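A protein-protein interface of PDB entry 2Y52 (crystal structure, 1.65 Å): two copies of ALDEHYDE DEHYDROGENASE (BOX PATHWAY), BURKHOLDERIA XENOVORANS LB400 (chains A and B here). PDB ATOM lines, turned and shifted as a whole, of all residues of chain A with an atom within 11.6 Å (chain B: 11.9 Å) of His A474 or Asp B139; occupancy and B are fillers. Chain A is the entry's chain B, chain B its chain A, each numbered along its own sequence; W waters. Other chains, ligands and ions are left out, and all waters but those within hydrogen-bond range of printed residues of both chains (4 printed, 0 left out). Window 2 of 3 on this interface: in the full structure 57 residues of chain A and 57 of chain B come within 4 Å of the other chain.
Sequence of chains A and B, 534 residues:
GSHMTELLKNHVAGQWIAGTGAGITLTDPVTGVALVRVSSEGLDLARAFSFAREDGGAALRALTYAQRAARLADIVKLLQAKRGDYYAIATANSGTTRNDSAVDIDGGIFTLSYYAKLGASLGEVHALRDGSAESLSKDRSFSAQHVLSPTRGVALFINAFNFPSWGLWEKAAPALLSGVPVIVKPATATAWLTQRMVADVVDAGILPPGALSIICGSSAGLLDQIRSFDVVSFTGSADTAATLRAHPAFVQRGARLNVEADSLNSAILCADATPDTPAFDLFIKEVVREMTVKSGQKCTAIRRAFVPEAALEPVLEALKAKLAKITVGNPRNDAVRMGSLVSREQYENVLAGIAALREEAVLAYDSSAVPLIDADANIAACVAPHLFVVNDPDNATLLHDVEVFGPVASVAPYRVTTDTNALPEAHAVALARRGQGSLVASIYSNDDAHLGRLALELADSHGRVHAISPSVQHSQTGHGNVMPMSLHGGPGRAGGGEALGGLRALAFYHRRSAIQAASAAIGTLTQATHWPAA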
ATOM      1  N   PRO A 278      -9.536  19.142 -11.621  1.00  0.00           N
ATOM      2  CA  PRO A 278      -9.501  19.201 -10.151  1.00  0.00           C
ATOM      3  C   PRO A 278     -10.838  19.618  -9.519  1.00  0.00           C
ATOM      4  O   PRO A 278     -11.272  19.055  -8.488  1.00  0.00           O
ATOM      5  CB  PRO A 278      -8.426  20.259  -9.859  1.00  0.00           C
ATOM      6  CG  PRO A 278      -7.624  20.351 -11.099  1.00  0.00           C
ATOM      7  CD  PRO A 278      -8.428  19.943 -12.233  1.00  0.00           C
ATOM      8  N   ALA A 279     -11.537  20.536 -10.186  1.00  0.00           N
ATOM      9  CA  ALA A 279     -12.774  21.050  -9.600  1.00  0.00           C
ATOM     10  C   ALA A 279     -13.866  19.984  -9.523  1.00  0.00           C
ATOM     11  O   ALA A 279     -14.730  20.105  -8.650  1.00  0.00           O
ATOM     12  CB  ALA A 279     -13.211  22.280 -10.345  1.00  0.00           C
ATOM     13  N   ASP A 281     -13.696  16.742  -8.579  1.00  0.00           N
ATOM     14  CA  ASP A 281     -13.606  15.985  -7.325  1.00  0.00           C
ATOM     15  C   ASP A 281     -13.982  16.866  -6.114  1.00  0.00           C
ATOM     16  O   ASP A 281     -14.520  16.326  -5.117  1.00  0.00           O
ATOM     17  CB  ASP A 281     -12.206  15.382  -7.088  1.00  0.00           C
ATOM     18  CG  ASP A 281     -12.210  14.338  -5.932  1.00  0.00           C
ATOM     19  OD1 ASP A 281     -13.093  13.431  -5.895  1.00  0.00           O
ATOM     20  OD2 ASP A 281     -11.342  14.452  -5.042  1.00  0.00           O
ATOM     21  N   LEU A 282     -13.638  18.169  -6.155  1.00  0.00           N
ATOM     22  CA  LEU A 282     -14.045  19.138  -5.062  1.00  0.00           C
ATOM     23  C   LEU A 282     -15.573  19.120  -4.914  1.00  0.00           C
ATOM     24  O   LEU A 282     -16.048  19.114  -3.792  1.00  0.00           O
ATOM     25  CB  LEU A 282     -13.458  20.561  -5.212  1.00  0.00           C
ATOM     26  CG  LEU A 282     -11.967  20.687  -5.429  1.00  0.00           C
ATOM     27  CD1 LEU A 282     -11.544  22.156  -5.781  1.00  0.00           C
ATOM     28  CD2 LEU A 282     -11.137  20.191  -4.210  1.00  0.00           C
ATOM     29  N   LYS A 285     -16.825  15.586  -3.395  1.00  0.00           N
ATOM     30  CA  LYS A 285     -16.475  15.615  -1.961  1.00  0.00           C
ATOM     31  C   LYS A 285     -17.426  16.488  -1.113  1.00  0.00           C
ATOM     32  O   LYS A 285     -17.876  16.090  -0.040  1.00  0.00           O
ATOM     33  CB  LYS A 285     -14.992  16.099  -1.794  1.00  0.00           C
ATOM     34  CG  LYS A 285     -13.954  15.021  -2.037  1.00  0.00           C
ATOM     35  CD  LYS A 285     -12.519  15.568  -1.667  1.00  0.00           C
ATOM     36  CE  LYS A 285     -11.473  14.574  -2.201  1.00  0.00           C
ATOM     37  NZ  LYS A 285     -10.117  14.995  -1.718  1.00  0.00           N
ATOM     38  N   GLU A 286     -17.788  17.652  -1.625  1.00  0.00           N
ATOM     39  CA  GLU A 286     -18.576  18.605  -0.812  1.00  0.00           C
ATOM     40  C   GLU A 286     -20.040  18.092  -0.713  1.00  0.00           C
ATOM     41  O   GLU A 286     -20.667  18.165   0.352  1.00  0.00           O
ATOM     42  CB  GLU A 286     -18.515  19.973  -1.466  1.00  0.00           C
ATOM     43  CG  GLU A 286     -18.877  21.117  -0.490  1.00  0.00           C
ATOM     44  CD  GLU A 286     -17.784  21.363   0.559  1.00  0.00           C
ATOM     45  OE1 GLU A 286     -16.649  20.847   0.359  1.00  0.00           O
ATOM     46  OE2 GLU A 286     -18.004  22.104   1.569  1.00  0.00           O
ATOM     47  N   ARG A 289     -20.038  15.288   1.757  1.00  0.00           N
ATOM     48  CA  ARG A 289     -19.922  15.911   3.106  1.00  0.00           C
ATOM     49  C   ARG A 289     -21.287  16.418   3.695  1.00  0.00           C
ATOM     50  O   ARG A 289     -21.589  16.238   4.883  1.00  0.00           O
ATOM     51  CB  ARG A 289     -18.880  17.013   3.150  1.00  0.00           C
ATOM     52  CG  ARG A 289     -18.377  17.358   4.553  1.00  0.00           C
ATOM     53  CD  ARG A 289     -17.069  18.244   4.564  1.00  0.00           C
ATOM     54  NE  ARG A 289     -17.228  19.298   5.585  1.00  0.00           N
ATOM     55  CZ  ARG A 289     -16.758  20.538   5.508  1.00  0.00           C
ATOM     56  NH1 ARG A 289     -16.077  20.960   4.449  1.00  0.00           N
ATOM     57  NH2 ARG A 289     -17.004  21.366   6.492  1.00  0.00           N
ATOM     58  N   SER A 445     -15.731  25.399  -9.878  1.00  0.00           N
ATOM     59  CA  SER A 445     -15.145  25.676 -11.194  1.00  0.00           C
ATOM     60  C   SER A 445     -13.620  25.677 -11.010  1.00  0.00           C
ATOM     61  O   SER A 445     -13.119  25.852  -9.914  1.00  0.00           O
ATOM     62  CB  SER A 445     -15.604  27.031 -11.691  1.00  0.00           C
ATOM     63  OG  SER A 445     -14.937  27.410 -12.939  1.00  0.00           O
ATOM     64  N   ASP A 448     -11.310  30.790 -11.324  1.00  0.00           N
ATOM     65  CA  ASP A 448     -11.606  31.766 -10.231  1.00  0.00           C
ATOM     66  C   ASP A 448     -12.327  33.037 -10.677  1.00  0.00           C
ATOM     67  O   ASP A 448     -13.217  33.513  -9.990  1.00  0.00           O
ATOM     68  CB  ASP A 448     -10.292  32.162  -9.556  1.00  0.00           C
ATOM     69  CG  ASP A 448      -9.787  31.077  -8.570  1.00  0.00           C
ATOM     70  OD1 ASP A 448     -10.465  30.015  -8.402  1.00  0.00           O
ATOM     71  OD2 ASP A 448      -8.714  31.266  -7.983  1.00  0.00           O
ATOM     72  N   HIS A 466     -21.253  30.378  -2.100  1.00  0.00           N
ATOM     73  CA  HIS A 466     -20.006  29.815  -1.573  1.00  0.00           C
ATOM     74  C   HIS A 466     -19.240  29.154  -2.713  1.00  0.00           C
ATOM     75  O   HIS A 466     -19.739  28.187  -3.285  1.00  0.00           O
ATOM     76  CB  HIS A 466     -20.350  28.750  -0.503  1.00  0.00           C
ATOM     77  CG  HIS A 466     -19.136  28.251   0.226  1.00  0.00           C
ATOM     78  ND1 HIS A 466     -18.403  27.147  -0.174  1.00  0.00           N
ATOM     79  CD2 HIS A 466     -18.475  28.779   1.304  1.00  0.00           C
ATOM     80  CE1 HIS A 466     -17.339  26.999   0.635  1.00  0.00           C
ATOM     81  NE2 HIS A 466     -17.380  27.978   1.540  1.00  0.00           N
ATOM     82  N   ALA A 467     -18.104  29.764  -3.141  1.00  0.00           N
ATOM     83  CA  ALA A 467     -17.511  29.362  -4.436  1.00  0.00           C
ATOM     84  C   ALA A 467     -16.264  28.543  -4.151  1.00  0.00           C
ATOM     85  O   ALA A 467     -15.377  29.001  -3.409  1.00  0.00           O
ATOM     86  CB  ALA A 467     -17.155  30.594  -5.332  1.00  0.00           C
ATOM     87  N   ILE A 468     -16.234  27.306  -4.676  1.00  0.00           N
ATOM     88  CA  ILE A 468     -15.143  26.368  -4.425  1.00  0.00           C
ATOM     89  C   ILE A 468     -14.328  26.097  -5.696  1.00  0.00           C
ATOM     90  O   ILE A 468     -14.868  25.778  -6.740  1.00  0.00           O
ATOM     91  CB  ILE A 468     -15.685  25.038  -3.772  1.00  0.00           C
ATOM     92  CG1 ILE A 468     -16.068  25.325  -2.276  1.00  0.00           C
ATOM     93  CG2 ILE A 468     -14.610  23.904  -3.871  1.00  0.00           C
ATOM     94  CD1 ILE A 468     -17.116  24.153  -1.790  1.00  0.00           C
ATOM     95  N   SER A 469     -12.998  26.239  -5.607  1.00  0.00           N
ATOM     96  CA  SER A 469     -12.136  26.026  -6.803  1.00  0.00           C
ATOM     97  C   SER A 469     -10.744  25.561  -6.288  1.00  0.00           C
ATOM     98  O   SER A 469     -10.437  25.648  -5.086  1.00  0.00           O
ATOM     99  CB  SER A 469     -11.850  27.330  -7.547  1.00  0.00           C
ATOM    100  OG  SER A 469     -11.608  28.337  -6.617  1.00  0.00           O
ATOM    101  N   PRO A 470      -9.893  25.059  -7.207  1.00  0.00           N
ATOM    102  CA  PRO A 470      -8.634  24.487  -6.690  1.00  0.00           C
ATOM    103  C   PRO A 470      -7.760  25.438  -5.884  1.00  0.00           C
ATOM    104  O   PRO A 470      -7.017  24.973  -4.994  1.00  0.00           O
ATOM    105  CB  PRO A 470      -7.897  24.067  -7.980  1.00  0.00           C
ATOM    106  CG  PRO A 470      -9.025  23.794  -8.950  1.00  0.00           C
ATOM    107  CD  PRO A 470     -10.102  24.784  -8.635  1.00  0.00           C
ATOM    108  N   SER A 471      -7.745  26.737  -6.204  1.00  0.00           N
ATOM    109  CA  SER A 471      -6.856  27.609  -5.432  1.00  0.00           C
ATOM    110  C   SER A 471      -7.237  27.741  -3.968  1.00  0.00           C
ATOM    111  O   SER A 471      -6.443  28.261  -3.159  1.00  0.00           O
ATOM    112  CB  SER A 471      -6.772  29.050  -5.997  1.00  0.00           C
ATOM    113  OG  SER A 471      -8.045  29.703  -5.845  1.00  0.00           O
ATOM    114  N   VAL A 472      -8.436  27.254  -3.608  1.00  0.00           N
ATOM    115  CA  VAL A 472      -8.868  27.343  -2.215  1.00  0.00           C
ATOM    116  C   VAL A 472      -9.287  25.956  -1.745  1.00  0.00           C
ATOM    117  O   VAL A 472     -10.034  25.825  -0.758  1.00  0.00           O
ATOM    118  CB  VAL A 472      -9.997  28.411  -2.036  1.00  0.00           C
ATOM    119  CG1 VAL A 472      -9.471  29.881  -2.366  1.00  0.00           C
ATOM    120  CG2 VAL A 472     -11.237  28.086  -2.898  1.00  0.00           C
ATOM    121  N   GLN A 473      -8.776  24.882  -2.388  1.00  0.00           N
ATOM    122  CA  GLN A 473      -9.060  23.547  -1.846  1.00  0.00           C
ATOM    123  C   GLN A 473      -8.661  23.391  -0.371  1.00  0.00           C
ATOM    124  O   GLN A 473      -9.284  22.680   0.384  1.00  0.00           O
ATOM    125  CB  GLN A 473      -8.418  22.455  -2.724  1.00  0.00           C
ATOM    126  CG  GLN A 473      -6.884  22.445  -2.755  1.00  0.00           C
ATOM    127  CD  GLN A 473      -6.372  20.997  -2.977  1.00  0.00           C
ATOM    128  OE1 GLN A 473      -6.937  20.250  -3.788  1.00  0.00           O
ATOM    129  NE2 GLN A 473      -5.363  20.589  -2.189  1.00  0.00           N
ATOM    130  N   HIS A 474      -7.607  24.087   0.032  1.00  0.00           N
ATOM    131  CA  HIS A 474      -7.071  23.957   1.351  1.00  0.00           C
ATOM    132  C   HIS A 474      -7.612  24.995   2.330  1.00  0.00           C
ATOM    133  O   HIS A 474      -7.377  24.876   3.519  1.00  0.00           O
ATOM    134  CB  HIS A 474      -5.546  24.151   1.296  1.00  0.00           C
ATOM    135  CG  HIS A 474      -5.175  25.553   0.884  1.00  0.00           C
ATOM    136  ND1 HIS A 474      -5.530  26.095  -0.343  1.00  0.00           N
ATOM    137  CD2 HIS A 474      -4.565  26.544   1.580  1.00  0.00           C
ATOM    138  CE1 HIS A 474      -5.103  27.347  -0.392  1.00  0.00           C
ATOM    139  NE2 HIS A 474      -4.523  27.644   0.765  1.00  0.00           N
ATOM    140  N   SER A 475      -8.377  25.982   1.858  1.00  0.00           N
ATOM    141  CA  SER A 475      -8.724  27.159   2.717  1.00  0.00           C
ATOM    142  C   SER A 475     -10.250  27.400   2.757  1.00  0.00           C
ATOM    143  O   SER A 475     -10.716  28.077   3.644  1.00  0.00           O
ATOM    144  CB  SER A 475      -8.040  28.464   2.230  1.00  0.00           C
ATOM    145  OG  SER A 475      -8.258  28.585   0.838  1.00  0.00           O
ATOM    146  N   GLN A 476     -10.975  26.954   1.745  1.00  0.00           N
ATOM    147  CA  GLN A 476     -12.434  27.217   1.665  1.00  0.00           C
ATOM    148  C   GLN A 476     -13.097  26.601   2.936  1.00  0.00           C
ATOM    149  O   GLN A 476     -12.711  25.501   3.373  1.00  0.00           O
ATOM    150  CB  GLN A 476     -12.981  26.641   0.334  1.00  0.00           C
ATOM    151  CG  GLN A 476     -13.021  25.053   0.262  1.00  0.00           C
ATOM    152  CD  GLN A 476     -14.366  24.400   0.715  1.00  0.00           C
ATOM    153  OE1 GLN A 476     -15.270  25.057   1.185  1.00  0.00           O
ATOM    154  NE2 GLN A 476     -14.471  23.078   0.503  1.00  0.00           N
ATOM    155  N   THR A 477     -14.104  27.317   3.501  1.00  0.00           N
ATOM    156  CA  THR A 477     -14.611  27.040   4.830  1.00  0.00           C
ATOM    157  C   THR A 477     -15.817  26.121   4.844  1.00  0.00           C
ATOM    158  O   THR A 477     -16.356  25.812   5.936  1.00  0.00           O
ATOM    159  CB  THR A 477     -14.952  28.384   5.524  1.00  0.00           C
ATOM    160  OG1 THR A 477     -15.784  29.205   4.640  1.00  0.00           O
ATOM    161  CG2 THR A 477     -13.672  29.074   5.825  1.00  0.00           C
ATOM    162  N   GLY A 478     -16.200  25.655   3.670  1.00  0.00           N
ATOM    163  CA  GLY A 478     -17.292  24.611   3.604  1.00  0.00           C
ATOM    164  C   GLY A 478     -18.654  25.207   3.218  1.00  0.00           C
ATOM    165  O   GLY A 478     -19.050  26.298   3.698  1.00  0.00           O
ATOM    166  N   ASN A 481     -20.986  25.182   6.418  1.00  0.00           N
ATOM    167  CA  ASN A 481     -20.481  25.740   7.671  1.00  0.00           C
ATOM    168  C   ASN A 481     -20.694  27.246   7.758  1.00  0.00           C
ATOM    169  O   ASN A 481     -20.280  27.987   6.855  1.00  0.00           O
ATOM    170  CB  ASN A 481     -18.965  25.459   7.818  1.00  0.00           C
ATOM    171  CG  ASN A 481     -18.643  23.969   7.965  1.00  0.00           C
ATOM    172  OD1 ASN A 481     -19.410  23.212   8.602  1.00  0.00           O
ATOM    173  ND2 ASN A 481     -17.488  23.531   7.396  1.00  0.00           N
ATOM    174  N   MET A 483     -19.757  30.710   8.883  1.00  0.00           N
ATOM    175  CA  MET A 483     -18.731  31.577   9.522  1.00  0.00           C
ATOM    176  C   MET A 483     -19.446  32.789  10.101  1.00  0.00           C
ATOM    177  O   MET A 483     -20.284  33.382   9.404  1.00  0.00           O
ATOM    178  CB  MET A 483     -17.671  31.996   8.466  1.00  0.00           C
ATOM    179  CG  MET A 483     -17.010  30.842   7.800  1.00  0.00           C
ATOM    180  SD  MET A 483     -16.007  29.864   8.946  1.00  0.00           S
ATOM    181  CE  MET A 483     -17.207  28.586   9.380  1.00  0.00           C
ATOM    182  N   GLU B 134     -13.204  40.748   3.695  1.00  0.00           N
ATOM    183  CA  GLU B 134     -12.710  40.256   4.946  1.00  0.00           C
ATOM    184  C   GLU B 134     -12.073  38.875   4.712  1.00  0.00           C
ATOM    185  O   GLU B 134     -12.623  38.031   3.981  1.00  0.00           O
ATOM    186  CB  GLU B 134     -13.931  40.264   5.913  1.00  0.00           C
ATOM    187  CG  GLU B 134     -13.967  39.302   7.007  1.00  0.00           C
ATOM    188  CD  GLU B 134     -14.758  39.882   8.199  1.00  0.00           C
ATOM    189  OE1 GLU B 134     -15.722  40.672   7.974  1.00  0.00           O
ATOM    190  OE2 GLU B 134     -14.352  39.544   9.300  1.00  0.00           O
ATOM    191  N   SER B 135     -10.868  38.637   5.277  1.00  0.00           N
ATOM    192  CA  SER B 135     -10.215  37.321   5.097  1.00  0.00           C
ATOM    193  C   SER B 135     -10.911  36.211   5.880  1.00  0.00           C
ATOM    194  O   SER B 135     -11.362  36.418   7.006  1.00  0.00           O
ATOM    195  CB  SER B 135      -8.726  37.400   5.489  1.00  0.00           C
ATOM    196  OG  SER B 135      -8.188  36.084   5.492  1.00  0.00           O
ATOM    197  N   LEU B 136     -11.020  35.025   5.290  1.00  0.00           N
ATOM    198  CA  LEU B 136     -11.597  33.890   6.011  1.00  0.00           C
ATOM    199  C   LEU B 136     -10.541  32.760   6.176  1.00  0.00           C
ATOM    200  O   LEU B 136     -10.917  31.620   6.472  1.00  0.00           O
ATOM    201  CB  LEU B 136     -12.797  33.320   5.253  1.00  0.00           C
ATOM    202  CG  LEU B 136     -14.084  34.132   5.140  1.00  0.00           C
ATOM    203  CD1 LEU B 136     -15.096  33.251   4.446  1.00  0.00           C
ATOM    204  CD2 LEU B 136     -14.586  34.512   6.513  1.00  0.00           C
ATOM    205  N   SER B 137      -9.253  33.074   5.972  1.00  0.00           N
ATOM    206  CA  SER B 137      -8.189  32.057   5.962  1.00  0.00           C
ATOM    207  C   SER B 137      -6.871  32.681   6.365  1.00  0.00           C
ATOM    208  O   SER B 137      -6.639  33.835   6.055  1.00  0.00           O
ATOM    209  CB  SER B 137      -7.987  31.448   4.572  1.00  0.00           C
ATOM    210  OG  SER B 137      -8.038  32.412   3.528  1.00  0.00           O
ATOM    211  N   LYS B 138      -5.994  31.891   7.026  1.00  0.00           N
ATOM    212  CA  LYS B 138      -4.685  32.379   7.477  1.00  0.00           C
ATOM    213  C   LYS B 138      -3.852  33.027   6.378  1.00  0.00           C
ATOM    214  O   LYS B 138      -3.215  34.064   6.621  1.00  0.00           O
ATOM    215  CB  LYS B 138      -3.861  31.247   8.122  1.00  0.00           C
ATOM    216  CG  LYS B 138      -3.178  31.599   9.476  1.00  0.00           C
ATOM    217  CD  LYS B 138      -2.933  33.094   9.757  1.00  0.00           C
ATOM    218  CE  LYS B 138      -4.258  33.825  10.214  1.00  0.00           C
ATOM    219  NZ  LYS B 138      -4.060  35.088  11.028  1.00  0.00           N
ATOM    220  N   ASP B 139      -3.847  32.428   5.192  1.00  0.00           N
ATOM    221  CA  ASP B 139      -3.018  32.867   4.062  1.00  0.00           C
ATOM    222  C   ASP B 139      -3.748  33.826   3.120  1.00  0.00           C
ATOM    223  O   ASP B 139      -3.255  34.140   2.042  1.00  0.00           O
ATOM    224  CB  ASP B 139      -2.471  31.655   3.251  1.00  0.00           C
ATOM    225  CG  ASP B 139      -3.543  30.898   2.482  1.00  0.00           C
ATOM    226  OD1 ASP B 139      -4.738  31.280   2.568  1.00  0.00           O
ATOM    227  OD2 ASP B 139      -3.189  29.939   1.728  1.00  0.00           O
ATOM    228  N   ARG B 140      -4.964  34.202   3.521  1.00  0.00           N
ATOM    229  CA  ARG B 140      -5.838  35.114   2.743  1.00  0.00           C
ATOM    230  C   ARG B 140      -6.223  34.712   1.315  1.00  0.00           C
ATOM    231  O   ARG B 140      -6.541  35.595   0.482  1.00  0.00           O
ATOM    232  CB  ARG B 140      -5.207  36.525   2.715  1.00  0.00           C
ATOM    233  CG  ARG B 140      -4.598  36.980   4.041  1.00  0.00           C
ATOM    234  CD  ARG B 140      -3.905  38.362   3.931  1.00  0.00           C
ATOM    235  NE  ARG B 140      -4.791  39.400   3.371  1.00  0.00           N
ATOM    236  CZ  ARG B 140      -5.640  40.133   4.093  1.00  0.00           C
ATOM    237  NH1 ARG B 140      -5.722  39.955   5.422  1.00  0.00           N
ATOM    238  NH2 ARG B 140      -6.400  41.053   3.489  1.00  0.00           N
ATOM    239  N   SER B 141      -6.212  33.416   1.009  1.00  0.00           N
ATOM    240  CA  SER B 141      -6.455  32.913  -0.299  1.00  0.00           C
ATOM    241  C   SER B 141      -8.002  32.803  -0.508  1.00  0.00           C
ATOM    242  O   SER B 141      -8.509  32.729  -1.655  1.00  0.00           O
ATOM    243  CB  SER B 141      -5.795  31.520  -0.485  1.00  0.00           C
ATOM    244  OG  SER B 141      -6.364  30.564   0.404  1.00  0.00           O
ATOM    245  N   PHE B 142      -8.712  32.764   0.621  1.00  0.00           N
ATOM    246  CA  PHE B 142     -10.185  32.661   0.636  1.00  0.00           C
ATOM    247  C   PHE B 142     -10.764  33.809   1.489  1.00  0.00           C
ATOM    248  O   PHE B 142     -10.264  34.057   2.621  1.00  0.00           O
ATOM    249  CB  PHE B 142     -10.646  31.264   1.204  1.00  0.00           C
ATOM    250  CG  PHE B 142     -12.138  30.917   0.963  1.00  0.00           C
ATOM    251  CD1 PHE B 142     -12.622  30.493  -0.322  1.00  0.00           C
ATOM    252  CD2 PHE B 142     -13.021  30.888   2.060  1.00  0.00           C
ATOM    253  CE1 PHE B 142     -14.027  30.136  -0.523  1.00  0.00           C
ATOM    254  CE2 PHE B 142     -14.393  30.543   1.889  1.00  0.00           C
ATOM    255  CZ  PHE B 142     -14.883  30.130   0.606  1.00  0.00           C
ATOM    256  N   SER B 143     -11.773  34.520   0.922  1.00  0.00           N
ATOM    257  CA  SER B 143     -12.321  35.769   1.515  1.00  0.00           C
ATOM    258  C   SER B 143     -13.832  35.906   1.321  1.00  0.00           C
ATOM    259  O   SER B 143     -14.478  35.166   0.555  1.00  0.00           O
ATOM    260  CB  SER B 143     -11.718  37.027   0.902  1.00  0.00           C
ATOM    261  OG  SER B 143     -10.350  37.159   1.199  1.00  0.00           O
ATOM    262  N   ALA B 144     -14.389  36.904   1.991  1.00  0.00           N
ATOM    263  CA  ALA B 144     -15.838  37.153   1.861  1.00  0.00           C
ATOM    264  C   ALA B 144     -16.087  38.636   1.578  1.00  0.00           C
ATOM    265  O   ALA B 144     -15.487  39.495   2.221  1.00  0.00           O
ATOM    266  CB  ALA B 144     -16.522  36.748   3.171  1.00  0.00           C
ATOM    267  N   ALA B 517     -15.350  33.236  -1.543  1.00  0.00           N
ATOM    268  CA  ALA B 517     -14.702  32.812  -2.783  1.00  0.00           C
ATOM    269  C   ALA B 517     -13.137  33.041  -2.738  1.00  0.00           C
ATOM    270  O   ALA B 517     -12.637  33.738  -1.913  1.00  0.00           O
ATOM    271  CB  ALA B 517     -15.333  33.531  -3.959  1.00  0.00           C
ATOM    272  N   ALA B 518     -12.437  32.430  -3.690  1.00  0.00           N
ATOM    273  CA  ALA B 518     -11.036  32.742  -3.945  1.00  0.00           C
ATOM    274  C   ALA B 518     -10.882  34.253  -4.003  1.00  0.00           C
ATOM    275  O   ALA B 518     -11.745  34.935  -4.548  1.00  0.00           O
ATOM    276  CB  ALA B 518     -10.645  32.146  -5.325  1.00  0.00           C
ATOM    277  N   SER B 519      -9.785  34.749  -3.465  1.00  0.00           N
ATOM    278  CA  SER B 519      -9.482  36.182  -3.447  1.00  0.00           C
ATOM    279  C   SER B 519      -9.459  36.858  -4.841  1.00  0.00           C
ATOM    280  O   SER B 519      -9.970  38.010  -4.960  1.00  0.00           O
ATOM    281  CB  SER B 519      -8.261  36.487  -2.564  1.00  0.00           C
ATOM    282  OG  SER B 519      -8.666  36.225  -1.178  1.00  0.00           O
ATOM    283  N   ALA B 520      -9.018  36.149  -5.889  1.00  0.00           N
ATOM    284  CA  ALA B 520      -9.225  36.647  -7.285  1.00  0.00           C
ATOM    285  C   ALA B 520     -10.704  36.925  -7.680  1.00  0.00           C
ATOM    286  O   ALA B 520     -10.987  37.959  -8.329  1.00  0.00           O
ATOM    287  CB  ALA B 520      -8.553  35.731  -8.345  1.00  0.00           C
HETATM  288  O   HOH W   1      -9.840  28.951   5.984  1.00  0.00           O
HETATM  289  O   HOH W   2      -7.591  33.712  -6.214  1.00  0.00           O
HETATM  290  O   HOH W   3     -13.351  30.020  -5.123  1.00  0.00           O
HETATM  291  O   HOH W   4      -7.235  31.958  -3.949  1.00  0.00           O
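OD2 of Asp B139 lies within hydrogen-bond range of NE2 of His A474.
OG of Ser B141 sits at hydrogen-bond distance from NE2 of His A474, at 3.5 Å.
The side-chain hydroxyl (OG) of Ser B141 sits at hydrogen-bond distance from the side-chain hydroxyl (OG) of Ser A475, 2.8 Å away.
The backbone NH (N) of Leu B136 is in hydrogen-bond range of the backbone carbonyl oxygen (O) of Phe B142 (2.9 Å).
O of Ser B141 sits at hydrogen-bond distance from N of Ser B519 (3.0 Å).
The side-chain carboxylate (OD1) of Asp A448 lies within hydrogen-bond range of the side-chain hydroxyl (OG) of Ser A469, at 2.7 Å.
OE1 of Gln A476 is in hydrogen-bond range of N of Gly A478 (2.7 Å).
The backbone carbonyl oxygen (O) of Thr A477 sits at hydrogen-bond distance from the side-chain amide nitrogen (ND2) of Asn A481, 2.9 Å away.
Phe B142 touches Ala A467.
Ala B517 touches Ala A467.
Ala B518 touches Ser A471.
Val A472 touches Ser B141 (CG1 to O, 3.1 Å).
Val A472 touches Ala B518.
Ser B137 touches Ser A475 (CB to CB, 3.8 Å).
Phe B142 touches Ser A475 (CB to OG, 3.6 Å).
Gln A476 touches Phe B142 (CA to CD2, 3.7 Å).
O of Leu B136 touches CG2 of Thr A477 (3.8 Å).
Thr A477 touches Phe B142.
Of the printed residues of chain B, His A474 touches Asp B139 and Ser B141.
Of chain A, only His A474 (2.8 Å) comes within 4 Å of Asp B139.
Ser A471 touches just one residue of chain B: Ala B518 (3.6 Å).
Printed residues of chain B within 4 Å of Val A472: Ser B141 (3.1 Å), Phe B142 (3.8 Å) and Ala B518 (3.6 Å).
No residue of chain B comes within 4 Å of Gln A473.
Ser A475 touches just these residues of chain B: Ser B137, Ser B141 and Phe B142.
Ser B137 touches just one residue of chain A: Ser A475.
No residue of chain A comes within 4 Å of Lys B138.
Of the printed residues of chain B, Thr A477 touches Leu B136 (3.8 Å) and Phe B142 (3.4 Å).
Of the printed residues of chain B, His A466 touches Phe B142.
Ser A469 touches none of the printed residues of chain B.
The nearest residue of chain A that does not touch Asp B139 is Ser A475 (4.4 Å).
Hydrophobic or aromatic side chains of chain B that line the printed part of chain A: Phe B142, Ala B517 and Ala B518.
Printed residues of chain A that touch a printed residue of chain B: Asp A448, His A466, Ala A467, Ser A471, Val A472, His A474, Ser A475, Gln A476 and Thr A477.
Hydrophobic or aromatic side chains of chain A that line the printed part of chain B: His A466, Ala A467, Val A472 and His A474.
Among the printed residues, 16 pairs touch across the chains.
Among the printed residues, no Asp or Glu carboxylate lies within 4 Å of a Lys or Arg side-chain nitrogen of the other chain.
No position is printed for both chains.
Of the 16 pairs that touch across the chains among the printed residues, none has its exchanged pair printed and touching as well.
Water W1 bridges the backbone carbonyl oxygen of Ser A475 (2.6 Å) and the backbone carbonyl oxygen of Leu B136 (2.9 Å).
Water W4 bridges O of Ser B141 (2.7 Å) and OG of Ser A471 (3.1 Å).
Water W2 lies within hydrogen-bond range of N of Ala B520 (2.8 Å) and OD2 of Asp A448 (3.2 Å).
Water W3 lies within hydrogen-bond range of the backbone carbonyl oxygen of Ala A467 (2.8 Å), the side-chain hydroxyl of Ser A469 (2.8 Å) and the backbone NH of Ala B518 (2.9 Å).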
